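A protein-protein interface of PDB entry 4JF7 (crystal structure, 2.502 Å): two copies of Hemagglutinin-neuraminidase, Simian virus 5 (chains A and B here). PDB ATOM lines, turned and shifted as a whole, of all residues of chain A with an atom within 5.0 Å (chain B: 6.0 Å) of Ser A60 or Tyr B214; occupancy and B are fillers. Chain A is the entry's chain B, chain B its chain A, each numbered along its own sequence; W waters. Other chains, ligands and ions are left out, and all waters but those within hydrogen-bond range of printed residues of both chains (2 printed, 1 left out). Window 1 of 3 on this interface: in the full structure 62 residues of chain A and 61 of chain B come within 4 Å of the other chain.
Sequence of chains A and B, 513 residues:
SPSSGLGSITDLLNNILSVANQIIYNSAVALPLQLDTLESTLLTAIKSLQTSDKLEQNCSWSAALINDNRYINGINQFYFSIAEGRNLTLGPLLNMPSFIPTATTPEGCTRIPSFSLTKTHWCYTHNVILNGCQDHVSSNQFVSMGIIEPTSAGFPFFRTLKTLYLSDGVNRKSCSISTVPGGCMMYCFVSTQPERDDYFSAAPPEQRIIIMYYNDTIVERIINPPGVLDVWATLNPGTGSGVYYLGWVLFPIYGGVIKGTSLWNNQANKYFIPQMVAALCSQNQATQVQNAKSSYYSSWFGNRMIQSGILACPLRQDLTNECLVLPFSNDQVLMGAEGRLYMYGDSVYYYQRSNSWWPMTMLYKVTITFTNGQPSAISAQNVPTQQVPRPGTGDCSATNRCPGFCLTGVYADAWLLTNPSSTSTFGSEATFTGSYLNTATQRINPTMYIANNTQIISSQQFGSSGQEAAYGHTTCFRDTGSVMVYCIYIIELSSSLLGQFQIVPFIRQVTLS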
ATOM      1  N   ASN A  58      -8.763  -7.621 -16.249  1.00  0.00           N
ATOM      2  CA  ASN A  58      -9.898  -6.711 -16.312  1.00  0.00           C
ATOM      3  C   ASN A  58     -11.246  -7.470 -16.298  1.00  0.00           C
ATOM      4  O   ASN A  58     -12.313  -6.859 -16.437  1.00  0.00           O
ATOM      5  CB  ASN A  58      -9.778  -5.873 -17.591  1.00  0.00           C
ATOM      6  CG  ASN A  58      -9.890  -4.384 -17.341  1.00  0.00           C
ATOM      7  OD1 ASN A  58     -10.953  -3.797 -17.530  1.00  0.00           O
ATOM      8  ND2 ASN A  58      -8.784  -3.757 -16.939  1.00  0.00           N
ATOM      9  N   CYS A  59     -11.205  -8.793 -16.137  1.00  0.00           N
ATOM     10  CA  CYS A  59     -12.424  -9.588 -16.278  1.00  0.00           C
ATOM     11  C   CYS A  59     -12.918 -10.207 -14.980  1.00  0.00           C
ATOM     12  O   CYS A  59     -12.128 -10.711 -14.188  1.00  0.00           O
ATOM     13  CB  CYS A  59     -12.238 -10.711 -17.315  1.00  0.00           C
ATOM     14  SG  CYS A  59     -11.851 -10.171 -18.994  1.00  0.00           S
ATOM     15  N   SER A  60     -14.235 -10.171 -14.786  1.00  0.00           N
ATOM     16  CA  SER A  60     -14.908 -11.056 -13.838  1.00  0.00           C
ATOM     17  C   SER A  60     -15.440 -12.205 -14.675  1.00  0.00           C
ATOM     18  O   SER A  60     -16.218 -11.997 -15.614  1.00  0.00           O
ATOM     19  CB  SER A  60     -16.067 -10.344 -13.132  1.00  0.00           C
ATOM     20  OG  SER A  60     -16.761 -11.235 -12.270  1.00  0.00           O
ATOM     21  N   TRP A  61     -15.004 -13.418 -14.362  1.00  0.00           N
ATOM     22  CA  TRP A  61     -15.343 -14.558 -15.209  1.00  0.00           C
ATOM     23  C   TRP A  61     -16.741 -15.111 -14.909  1.00  0.00           C
ATOM     24  O   TRP A  61     -17.225 -15.018 -13.785  1.00  0.00           O
ATOM     25  CB  TRP A  61     -14.287 -15.667 -15.090  1.00  0.00           C
ATOM     26  CG  TRP A  61     -12.882 -15.252 -15.471  1.00  0.00           C
ATOM     27  CD1 TRP A  61     -11.783 -15.212 -14.650  1.00  0.00           C
ATOM     28  CD2 TRP A  61     -12.428 -14.821 -16.767  1.00  0.00           C
ATOM     29  NE1 TRP A  61     -10.680 -14.783 -15.355  1.00  0.00           N
ATOM     30  CE2 TRP A  61     -11.048 -14.535 -16.654  1.00  0.00           C
ATOM     31  CE3 TRP A  61     -13.052 -14.647 -18.007  1.00  0.00           C
ATOM     32  CZ2 TRP A  61     -10.284 -14.089 -17.738  1.00  0.00           C
ATOM     33  CZ3 TRP A  61     -12.289 -14.202 -19.082  1.00  0.00           C
ATOM     34  CH2 TRP A  61     -10.921 -13.929 -18.939  1.00  0.00           C
ATOM     35  N   SER A  62     -17.379 -15.677 -15.931  1.00  0.00           N
ATOM     36  CA  SER A  62     -18.634 -16.395 -15.778  1.00  0.00           C
ATOM     37  C   SER A  62     -18.565 -17.467 -14.693  1.00  0.00           C
ATOM     38  O   SER A  62     -19.580 -17.824 -14.102  1.00  0.00           O
ATOM     39  CB  SER A  62     -19.026 -17.045 -17.101  1.00  0.00           C
ATOM     40  OG  SER A  62     -19.691 -16.118 -17.929  1.00  0.00           O
ATOM     41  N   ALA A  64     -17.578 -17.026 -11.916  1.00  0.00           N
ATOM     42  CA  ALA A  64     -18.042 -16.367 -10.707  1.00  0.00           C
ATOM     43  C   ALA A  64     -19.492 -16.745 -10.438  1.00  0.00           C
ATOM     44  O   ALA A  64     -19.907 -16.839  -9.285  1.00  0.00           O
ATOM     45  CB  ALA A  64     -17.889 -14.829 -10.820  1.00  0.00           C
ATOM     46  N   LYS A 162     -25.087  -9.190 -10.629  1.00  0.00           N
ATOM     47  CA  LYS A 162     -25.409  -8.268 -11.700  1.00  0.00           C
ATOM     48  C   LYS A 162     -26.829  -7.785 -11.544  1.00  0.00           C
ATOM     49  O   LYS A 162     -27.714  -8.524 -11.112  1.00  0.00           O
ATOM     50  CB  LYS A 162     -25.252  -8.885 -13.094  1.00  0.00           C
ATOM     51  CG  LYS A 162     -25.152  -7.800 -14.195  1.00  0.00           C
ATOM     52  CD  LYS A 162     -25.260  -8.352 -15.615  1.00  0.00           C
ATOM     53  CE  LYS A 162     -24.138  -9.322 -15.931  1.00  0.00           C
ATOM     54  NZ  LYS A 162     -22.776  -8.777 -15.669  1.00  0.00           N
ATOM     55  N   TYR A 214     -24.370 -13.136 -18.157  1.00  0.00           N
ATOM     56  CA  TYR A 214     -23.401 -12.578 -17.220  1.00  0.00           C
ATOM     57  C   TYR A 214     -22.299 -11.782 -17.921  1.00  0.00           C
ATOM     58  O   TYR A 214     -21.735 -10.845 -17.339  1.00  0.00           O
ATOM     59  CB  TYR A 214     -22.781 -13.644 -16.301  1.00  0.00           C
ATOM     60  CG  TYR A 214     -21.938 -13.007 -15.214  1.00  0.00           C
ATOM     61  CD1 TYR A 214     -22.540 -12.439 -14.091  1.00  0.00           C
ATOM     62  CD2 TYR A 214     -20.548 -12.919 -15.332  1.00  0.00           C
ATOM     63  CE1 TYR A 214     -21.789 -11.830 -13.103  1.00  0.00           C
ATOM     64  CE2 TYR A 214     -19.780 -12.307 -14.342  1.00  0.00           C
ATOM     65  CZ  TYR A 214     -20.409 -11.763 -13.227  1.00  0.00           C
ATOM     66  OH  TYR A 214     -19.666 -11.149 -12.234  1.00  0.00           O
ATOM     67  N   ASP A 216     -22.623  -9.738 -20.132  1.00  0.00           N
ATOM     68  CA  ASP A 216     -23.247  -8.452 -20.468  1.00  0.00           C
ATOM     69  C   ASP A 216     -23.955  -8.420 -21.823  1.00  0.00           C
ATOM     70  O   ASP A 216     -24.570  -7.421 -22.180  1.00  0.00           O
ATOM     71  CB  ASP A 216     -22.296  -7.261 -20.280  1.00  0.00           C
ATOM     72  CG  ASP A 216     -21.752  -7.176 -18.857  1.00  0.00           C
ATOM     73  OD1 ASP A 216     -20.514  -7.081 -18.700  1.00  0.00           O
ATOM     74  OD2 ASP A 216     -22.559  -7.209 -17.896  1.00  0.00           O
ATOM     75  N   ASN B  58     -16.745 -15.863 -21.673  1.00  0.00           N
ATOM     76  CA  ASN B  58     -16.844 -16.016 -20.222  1.00  0.00           C
ATOM     77  C   ASN B  58     -16.476 -14.755 -19.449  1.00  0.00           C
ATOM     78  O   ASN B  58     -16.344 -14.794 -18.232  1.00  0.00           O
ATOM     79  CB  ASN B  58     -15.951 -17.163 -19.729  1.00  0.00           C
ATOM     80  CG  ASN B  58     -16.212 -18.463 -20.451  1.00  0.00           C
ATOM     81  OD1 ASN B  58     -16.622 -18.464 -21.611  1.00  0.00           O
ATOM     82  ND2 ASN B  58     -15.976 -19.583 -19.771  1.00  0.00           N
ATOM     83  N   CYS B  59     -16.309 -13.640 -20.148  1.00  0.00           N
ATOM     84  CA  CYS B  59     -15.779 -12.436 -19.513  1.00  0.00           C
ATOM     85  C   CYS B  59     -16.789 -11.297 -19.355  1.00  0.00           C
ATOM     86  O   CYS B  59     -17.368 -10.830 -20.331  1.00  0.00           O
ATOM     87  CB  CYS B  59     -14.558 -11.932 -20.290  1.00  0.00           C
ATOM     88  SG  CYS B  59     -13.770 -10.462 -19.589  1.00  0.00           S
ATOM     89  N   SER B  60     -17.000 -10.855 -18.119  1.00  0.00           N
ATOM     90  CA  SER B  60     -17.699  -9.597 -17.878  1.00  0.00           C
ATOM     91  C   SER B  60     -16.661  -8.489 -17.742  1.00  0.00           C
ATOM     92  O   SER B  60     -16.039  -8.338 -16.689  1.00  0.00           O
ATOM     93  CB  SER B  60     -18.562  -9.668 -16.623  1.00  0.00           C
ATOM     94  OG  SER B  60     -19.244  -8.441 -16.423  1.00  0.00           O
ATOM     95  N   TRP B  61     -16.489  -7.726 -18.822  1.00  0.00           N
ATOM     96  CA  TRP B  61     -15.403  -6.754 -18.971  1.00  0.00           C
ATOM     97  C   TRP B  61     -15.594  -5.534 -18.069  1.00  0.00           C
ATOM     98  O   TRP B  61     -16.679  -4.954 -18.025  1.00  0.00           O
ATOM     99  CB  TRP B  61     -15.308  -6.318 -20.439  1.00  0.00           C
ATOM    100  CG  TRP B  61     -13.992  -5.701 -20.842  1.00  0.00           C
ATOM    101  CD1 TRP B  61     -12.757  -5.969 -20.316  1.00  0.00           C
ATOM    102  CD2 TRP B  61     -13.786  -4.711 -21.860  1.00  0.00           C
ATOM    103  NE1 TRP B  61     -11.799  -5.207 -20.944  1.00  0.00           N
ATOM    104  CE2 TRP B  61     -12.405  -4.427 -21.895  1.00  0.00           C
ATOM    105  CE3 TRP B  61     -14.636  -4.037 -22.746  1.00  0.00           C
ATOM    106  CZ2 TRP B  61     -11.856  -3.498 -22.779  1.00  0.00           C
ATOM    107  CZ3 TRP B  61     -14.091  -3.116 -23.622  1.00  0.00           C
ATOM    108  CH2 TRP B  61     -12.713  -2.854 -23.632  1.00  0.00           C
ATOM    109  N   SER B  62     -14.535  -5.142 -17.364  1.00  0.00           N
ATOM    110  CA  SER B  62     -14.614  -4.056 -16.386  1.00  0.00           C
ATOM    111  C   SER B  62     -14.965  -2.681 -16.958  1.00  0.00           C
ATOM    112  O   SER B  62     -15.152  -1.737 -16.196  1.00  0.00           O
ATOM    113  CB  SER B  62     -13.335  -3.957 -15.547  1.00  0.00           C
ATOM    114  OG  SER B  62     -13.228  -5.034 -14.634  1.00  0.00           O
ATOM    115  N   ALA B  64     -17.757  -2.375 -18.027  1.00  0.00           N
ATOM    116  CA  ALA B  64     -19.163  -2.360 -17.635  1.00  0.00           C
ATOM    117  C   ALA B  64     -19.130  -1.369 -16.518  1.00  0.00           C
ATOM    118  O   ALA B  64     -19.895  -0.406 -16.493  1.00  0.00           O
ATOM    119  CB  ALA B  64     -19.627  -3.725 -17.105  1.00  0.00           C
ATOM    120  N   LEU B  65     -18.185  -1.596 -15.608  1.00  0.00           N
ATOM    121  CA  LEU B  65     -17.961  -0.739 -14.447  1.00  0.00           C
ATOM    122  C   LEU B  65     -17.572   0.667 -14.910  1.00  0.00           C
ATOM    123  O   LEU B  65     -16.595   1.243 -14.411  1.00  0.00           O
ATOM    124  CB  LEU B  65     -16.878  -1.343 -13.520  1.00  0.00           C
ATOM    125  CG  LEU B  65     -16.819  -1.003 -12.020  1.00  0.00           C
ATOM    126  CD1 LEU B  65     -17.738  -1.896 -11.200  1.00  0.00           C
ATOM    127  CD2 LEU B  65     -15.381  -1.054 -11.492  1.00  0.00           C
ATOM    128  N   MET B 145     -20.582  -2.388  -5.294  1.00  0.00           N
ATOM    129  CA  MET B 145     -20.022  -1.440  -6.234  1.00  0.00           C
ATOM    130  C   MET B 145     -20.869  -1.444  -7.497  1.00  0.00           C
ATOM    131  O   MET B 145     -21.488  -2.445  -7.835  1.00  0.00           O
ATOM    132  CB  MET B 145     -18.543  -1.753  -6.535  1.00  0.00           C
ATOM    133  CG  MET B 145     -18.302  -3.028  -7.327  1.00  0.00           C
ATOM    134  SD  MET B 145     -16.579  -3.588  -7.415  1.00  0.00           S
ATOM    135  CE  MET B 145     -16.299  -4.149  -5.744  1.00  0.00           C
ATOM    136  N   LEU B 161     -23.196  -3.683  -9.655  1.00  0.00           N
ATOM    137  CA  LEU B 161     -22.486  -4.646 -10.495  1.00  0.00           C
ATOM    138  C   LEU B 161     -21.812  -5.776  -9.692  1.00  0.00           C
ATOM    139  O   LEU B 161     -21.425  -6.807 -10.246  1.00  0.00           O
ATOM    140  CB  LEU B 161     -21.474  -3.924 -11.388  1.00  0.00           C
ATOM    141  CG  LEU B 161     -22.133  -2.972 -12.382  1.00  0.00           C
ATOM    142  CD1 LEU B 161     -21.085  -2.261 -13.221  1.00  0.00           C
ATOM    143  CD2 LEU B 161     -23.105  -3.734 -13.261  1.00  0.00           C
ATOM    144  N   LYS B 162     -21.656  -5.567  -8.390  1.00  0.00           N
ATOM    145  CA  LYS B 162     -21.208  -6.623  -7.501  1.00  0.00           C
ATOM    146  C   LYS B 162     -21.626  -6.322  -6.067  1.00  0.00           C
ATOM    147  O   LYS B 162     -21.613  -5.171  -5.654  1.00  0.00           O
ATOM    148  CB  LYS B 162     -19.697  -6.785  -7.563  1.00  0.00           C
ATOM    149  CG  LYS B 162     -19.215  -8.121  -7.022  1.00  0.00           C
ATOM    150  CD  LYS B 162     -17.686  -8.204  -6.986  1.00  0.00           C
ATOM    151  CE  LYS B 162     -17.061  -8.094  -8.389  1.00  0.00           C
ATOM    152  NZ  LYS B 162     -17.419  -9.198  -9.354  1.00  0.00           N
ATOM    153  N   GLY B 182     -10.771   0.091 -10.625  1.00  0.00           N
ATOM    154  CA  GLY B 182     -11.136  -1.316 -10.690  1.00  0.00           C
ATOM    155  C   GLY B 182     -11.921  -1.857  -9.511  1.00  0.00           C
ATOM    156  O   GLY B 182     -12.366  -2.999  -9.532  1.00  0.00           O
ATOM    157  N   GLY B 183     -12.108  -1.051  -8.473  1.00  0.00           N
ATOM    158  CA  GLY B 183     -12.862  -1.526  -7.331  1.00  0.00           C
ATOM    159  C   GLY B 183     -12.929  -0.580  -6.154  1.00  0.00           C
ATOM    160  O   GLY B 183     -13.074   0.628  -6.324  1.00  0.00           O
ATOM    161  N   MET B 212     -11.171  -4.739  -2.734  1.00  0.00           N
ATOM    162  CA  MET B 212     -12.102  -5.585  -3.466  1.00  0.00           C
ATOM    163  C   MET B 212     -12.213  -5.124  -4.914  1.00  0.00           C
ATOM    164  O   MET B 212     -12.594  -3.985  -5.190  1.00  0.00           O
ATOM    165  CB  MET B 212     -13.467  -5.553  -2.786  1.00  0.00           C
ATOM    166  CG  MET B 212     -13.424  -6.117  -1.353  1.00  0.00           C
ATOM    167  SD  MET B 212     -14.700  -5.447  -0.237  1.00  0.00           S
ATOM    168  CE  MET B 212     -14.103  -3.751  -0.114  1.00  0.00           C
ATOM    169  N   TYR B 213     -11.873  -6.007  -5.843  1.00  0.00           N
ATOM    170  CA  TYR B 213     -11.888  -5.617  -7.243  1.00  0.00           C
ATOM    171  C   TYR B 213     -13.064  -6.201  -7.970  1.00  0.00           C
ATOM    172  O   TYR B 213     -13.630  -7.184  -7.529  1.00  0.00           O
ATOM    173  CB  TYR B 213     -10.592  -6.022  -7.936  1.00  0.00           C
ATOM    174  CG  TYR B 213      -9.384  -5.245  -7.485  1.00  0.00           C
ATOM    175  CD1 TYR B 213      -9.217  -3.921  -7.854  1.00  0.00           C
ATOM    176  CD2 TYR B 213      -8.397  -5.838  -6.701  1.00  0.00           C
ATOM    177  CE1 TYR B 213      -8.093  -3.199  -7.459  1.00  0.00           C
ATOM    178  CE2 TYR B 213      -7.264  -5.120  -6.296  1.00  0.00           C
ATOM    179  CZ  TYR B 213      -7.122  -3.800  -6.683  1.00  0.00           C
ATOM    180  OH  TYR B 213      -6.016  -3.060  -6.301  1.00  0.00           O
ATOM    181  N   TYR B 214     -13.436  -5.573  -9.083  1.00  0.00           N
ATOM    182  CA  TYR B 214     -14.475  -6.102  -9.961  1.00  0.00           C
ATOM    183  C   TYR B 214     -14.116  -7.492 -10.490  1.00  0.00           C
ATOM    184  O   TYR B 214     -15.007  -8.300 -10.769  1.00  0.00           O
ATOM    185  CB  TYR B 214     -14.791  -5.157 -11.141  1.00  0.00           C
ATOM    186  CG  TYR B 214     -15.969  -5.681 -11.938  1.00  0.00           C
ATOM    187  CD1 TYR B 214     -17.266  -5.571 -11.434  1.00  0.00           C
ATOM    188  CD2 TYR B 214     -15.789  -6.334 -13.165  1.00  0.00           C
ATOM    189  CE1 TYR B 214     -18.344  -6.084 -12.121  1.00  0.00           C
ATOM    190  CE2 TYR B 214     -16.872  -6.852 -13.866  1.00  0.00           C
ATOM    191  CZ  TYR B 214     -18.148  -6.720 -13.332  1.00  0.00           C
ATOM    192  OH  TYR B 214     -19.245  -7.216 -13.995  1.00  0.00           O
ATOM    193  N   ASN B 215     -12.818  -7.767 -10.626  1.00  0.00           N
ATOM    194  CA  ASN B 215     -12.360  -9.078 -11.100  1.00  0.00           C
ATOM    195  C   ASN B 215     -12.390 -10.168 -10.034  1.00  0.00           C
ATOM    196  O   ASN B 215     -11.844 -11.246 -10.251  1.00  0.00           O
ATOM    197  CB  ASN B 215     -10.958  -8.986 -11.708  1.00  0.00           C
ATOM    198  CG  ASN B 215      -9.880  -8.690 -10.673  1.00  0.00           C
ATOM    199  OD1 ASN B 215     -10.098  -8.832  -9.466  1.00  0.00           O
ATOM    200  ND2 ASN B 215      -8.700  -8.270 -11.149  1.00  0.00           N
ATOM    201  N   ASP B 216     -12.966  -9.842  -8.873  1.00  0.00           N
ATOM    202  CA  ASP B 216     -13.266 -10.804  -7.803  1.00  0.00           C
ATOM    203  C   ASP B 216     -12.094 -11.118  -6.881  1.00  0.00           C
ATOM    204  O   ASP B 216     -12.223 -11.875  -5.926  1.00  0.00           O
ATOM    205  CB  ASP B 216     -13.893 -12.080  -8.359  1.00  0.00           C
ATOM    206  CG  ASP B 216     -15.205 -11.804  -9.042  1.00  0.00           C
ATOM    207  OD1 ASP B 216     -15.321 -12.050 -10.266  1.00  0.00           O
ATOM    208  OD2 ASP B 216     -16.115 -11.312  -8.342  1.00  0.00           O
ATOM    209  N   THR B 217     -10.957 -10.513  -7.165  1.00  0.00           N
ATOM    210  CA  THR B 217      -9.862 -10.521  -6.227  1.00  0.00           C
ATOM    211  C   THR B 217     -10.221  -9.706  -4.984  1.00  0.00           C
ATOM    212  O   THR B 217     -10.782  -8.607  -5.081  1.00  0.00           O
ATOM    213  CB  THR B 217      -8.607  -9.955  -6.880  1.00  0.00           C
ATOM    214  OG1 THR B 217      -8.169 -10.870  -7.889  1.00  0.00           O
ATOM    215  CG2 THR B 217      -7.499  -9.748  -5.847  1.00  0.00           C
HETATM  216  O   HOH W   1     -21.781  -7.741 -13.332  1.00  0.00           O
HETATM  217  O   HOH W   2     -13.841 -13.845 -11.932  1.00  0.00           O
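The side-chain hydroxyl of Ser B62 lies within hydrogen-bond range of the backbone carbonyl oxygen of Asn A58 (2.7 Å). O of Asn B58 lies within hydrogen-bond range of N of Ser A62 (2.7 Å). The side-chain hydroxyl of Ser B60 lies within hydrogen-bond range of the side-chain carboxylate of Asp A216, at 2.9 Å. SG of Cys A59 forms a disulfide with SG of Cys B59 (2.0 Å). The backbone carbonyl oxygen of Ser A60 is in hydrogen-bond range of the backbone NH of Ser B60, 2.9 Å away. OD1 of Asp B216 lies within hydrogen-bond range of OG of Ser A60.
NZ of Lys A162 sits at hydrogen-bond distance from O of Tyr A214 (2.9 Å). The side-chain amino group (NZ) of Lys B162 is in salt-bridge range of the side-chain carboxylate (OD2) of Asp B216 (2.7 Å). The backbone NH of Tyr B214 sits at hydrogen-bond distance from the backbone carbonyl oxygen of Gly B182, at 2.8 Å. OD1 of Asn B215 sits at hydrogen-bond distance from N of Thr B217 (3.0 Å). The side-chain amino group (NZ) of Lys B162 sits at hydrogen-bond distance from the backbone carbonyl oxygen (O) of Tyr B214, 2.9 Å away. The side-chain hydroxyl (OG) of Ser B60 lies within hydrogen-bond range of the side-chain hydroxyl (OH) of Tyr B214 (2.7 Å).
Among the printed residues, pairs that only touch across the chains: Trp A61 with Asn B58 (3.2 Å), Cys A59 with Asn B215 (3.2 Å), Ser A60 with Tyr B214 (3.3 Å), Trp A61 with Cys B59 (3.4 Å), Tyr A214 with Ser B60 (3.5 Å), Ser A60 with Lys B162 (3.6 Å), Lys A162 with Ser B60 (3.6 Å), Asn A58 with Trp B61 (3.8 Å), Asp A216 with Ala B64 (3.8 Å), Ala A64 with Asp B216 (3.8 Å), Ser A60 with Asn B58 (3.8 Å), Cys A59 with Ser B60 (3.8 Å) and Ser A60 with Cys B59 (3.8 Å).
Ser A60 touches just these residues of chain B: Asn B58, Cys B59, Ser B60, Lys B162, Tyr B214 and Asp B216. Printed residues of chain A within 4 Å of Asn B58: Ser A60, Trp A61 and Ser A62. Printed residues of chain A within 4 Å of Cys B59: Cys A59 (2.0 Å), Ser A60 (3.8 Å) and Trp A61 (3.4 Å). Tyr B214 touches just one residue of chain A: Ser A60 (3.3 Å).
Among the printed residues, no Asp or Glu carboxylate lies within 4 Å of a Lys or Arg side-chain nitrogen of the other chain.
Asn A58 touches Trp B61, and with the chains exchanged Trp A61 touches Asn B58. Asn A58 touches Ser B62, and with the chains exchanged Ser A62 touches Asn B58. Cys A59 touches Ser B60, and with the chains exchanged Ser A60 touches Cys B59. Trp A61 touches Cys B59, but with the chains exchanged Cys A59 does not touch Trp B61 (4.5 Å). Positions printed for both chains: 58, 59, 60, 61, 62, 64, 162, 214 and 216. Of the 19 pairs that touch across the chains among the printed residues, 16 have their exchanged pair printed and touching as well.
Water W1 lies within hydrogen-bond range of the side-chain hydroxyl of Tyr B214 (2.7 Å), the side-chain amino group of Lys A162 (2.7 Å) and the backbone carbonyl oxygen of Leu B161 (3.2 Å). Water W2 bridges the backbone NH of Trp A61 and the side-chain carboxylate of Asp B216.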
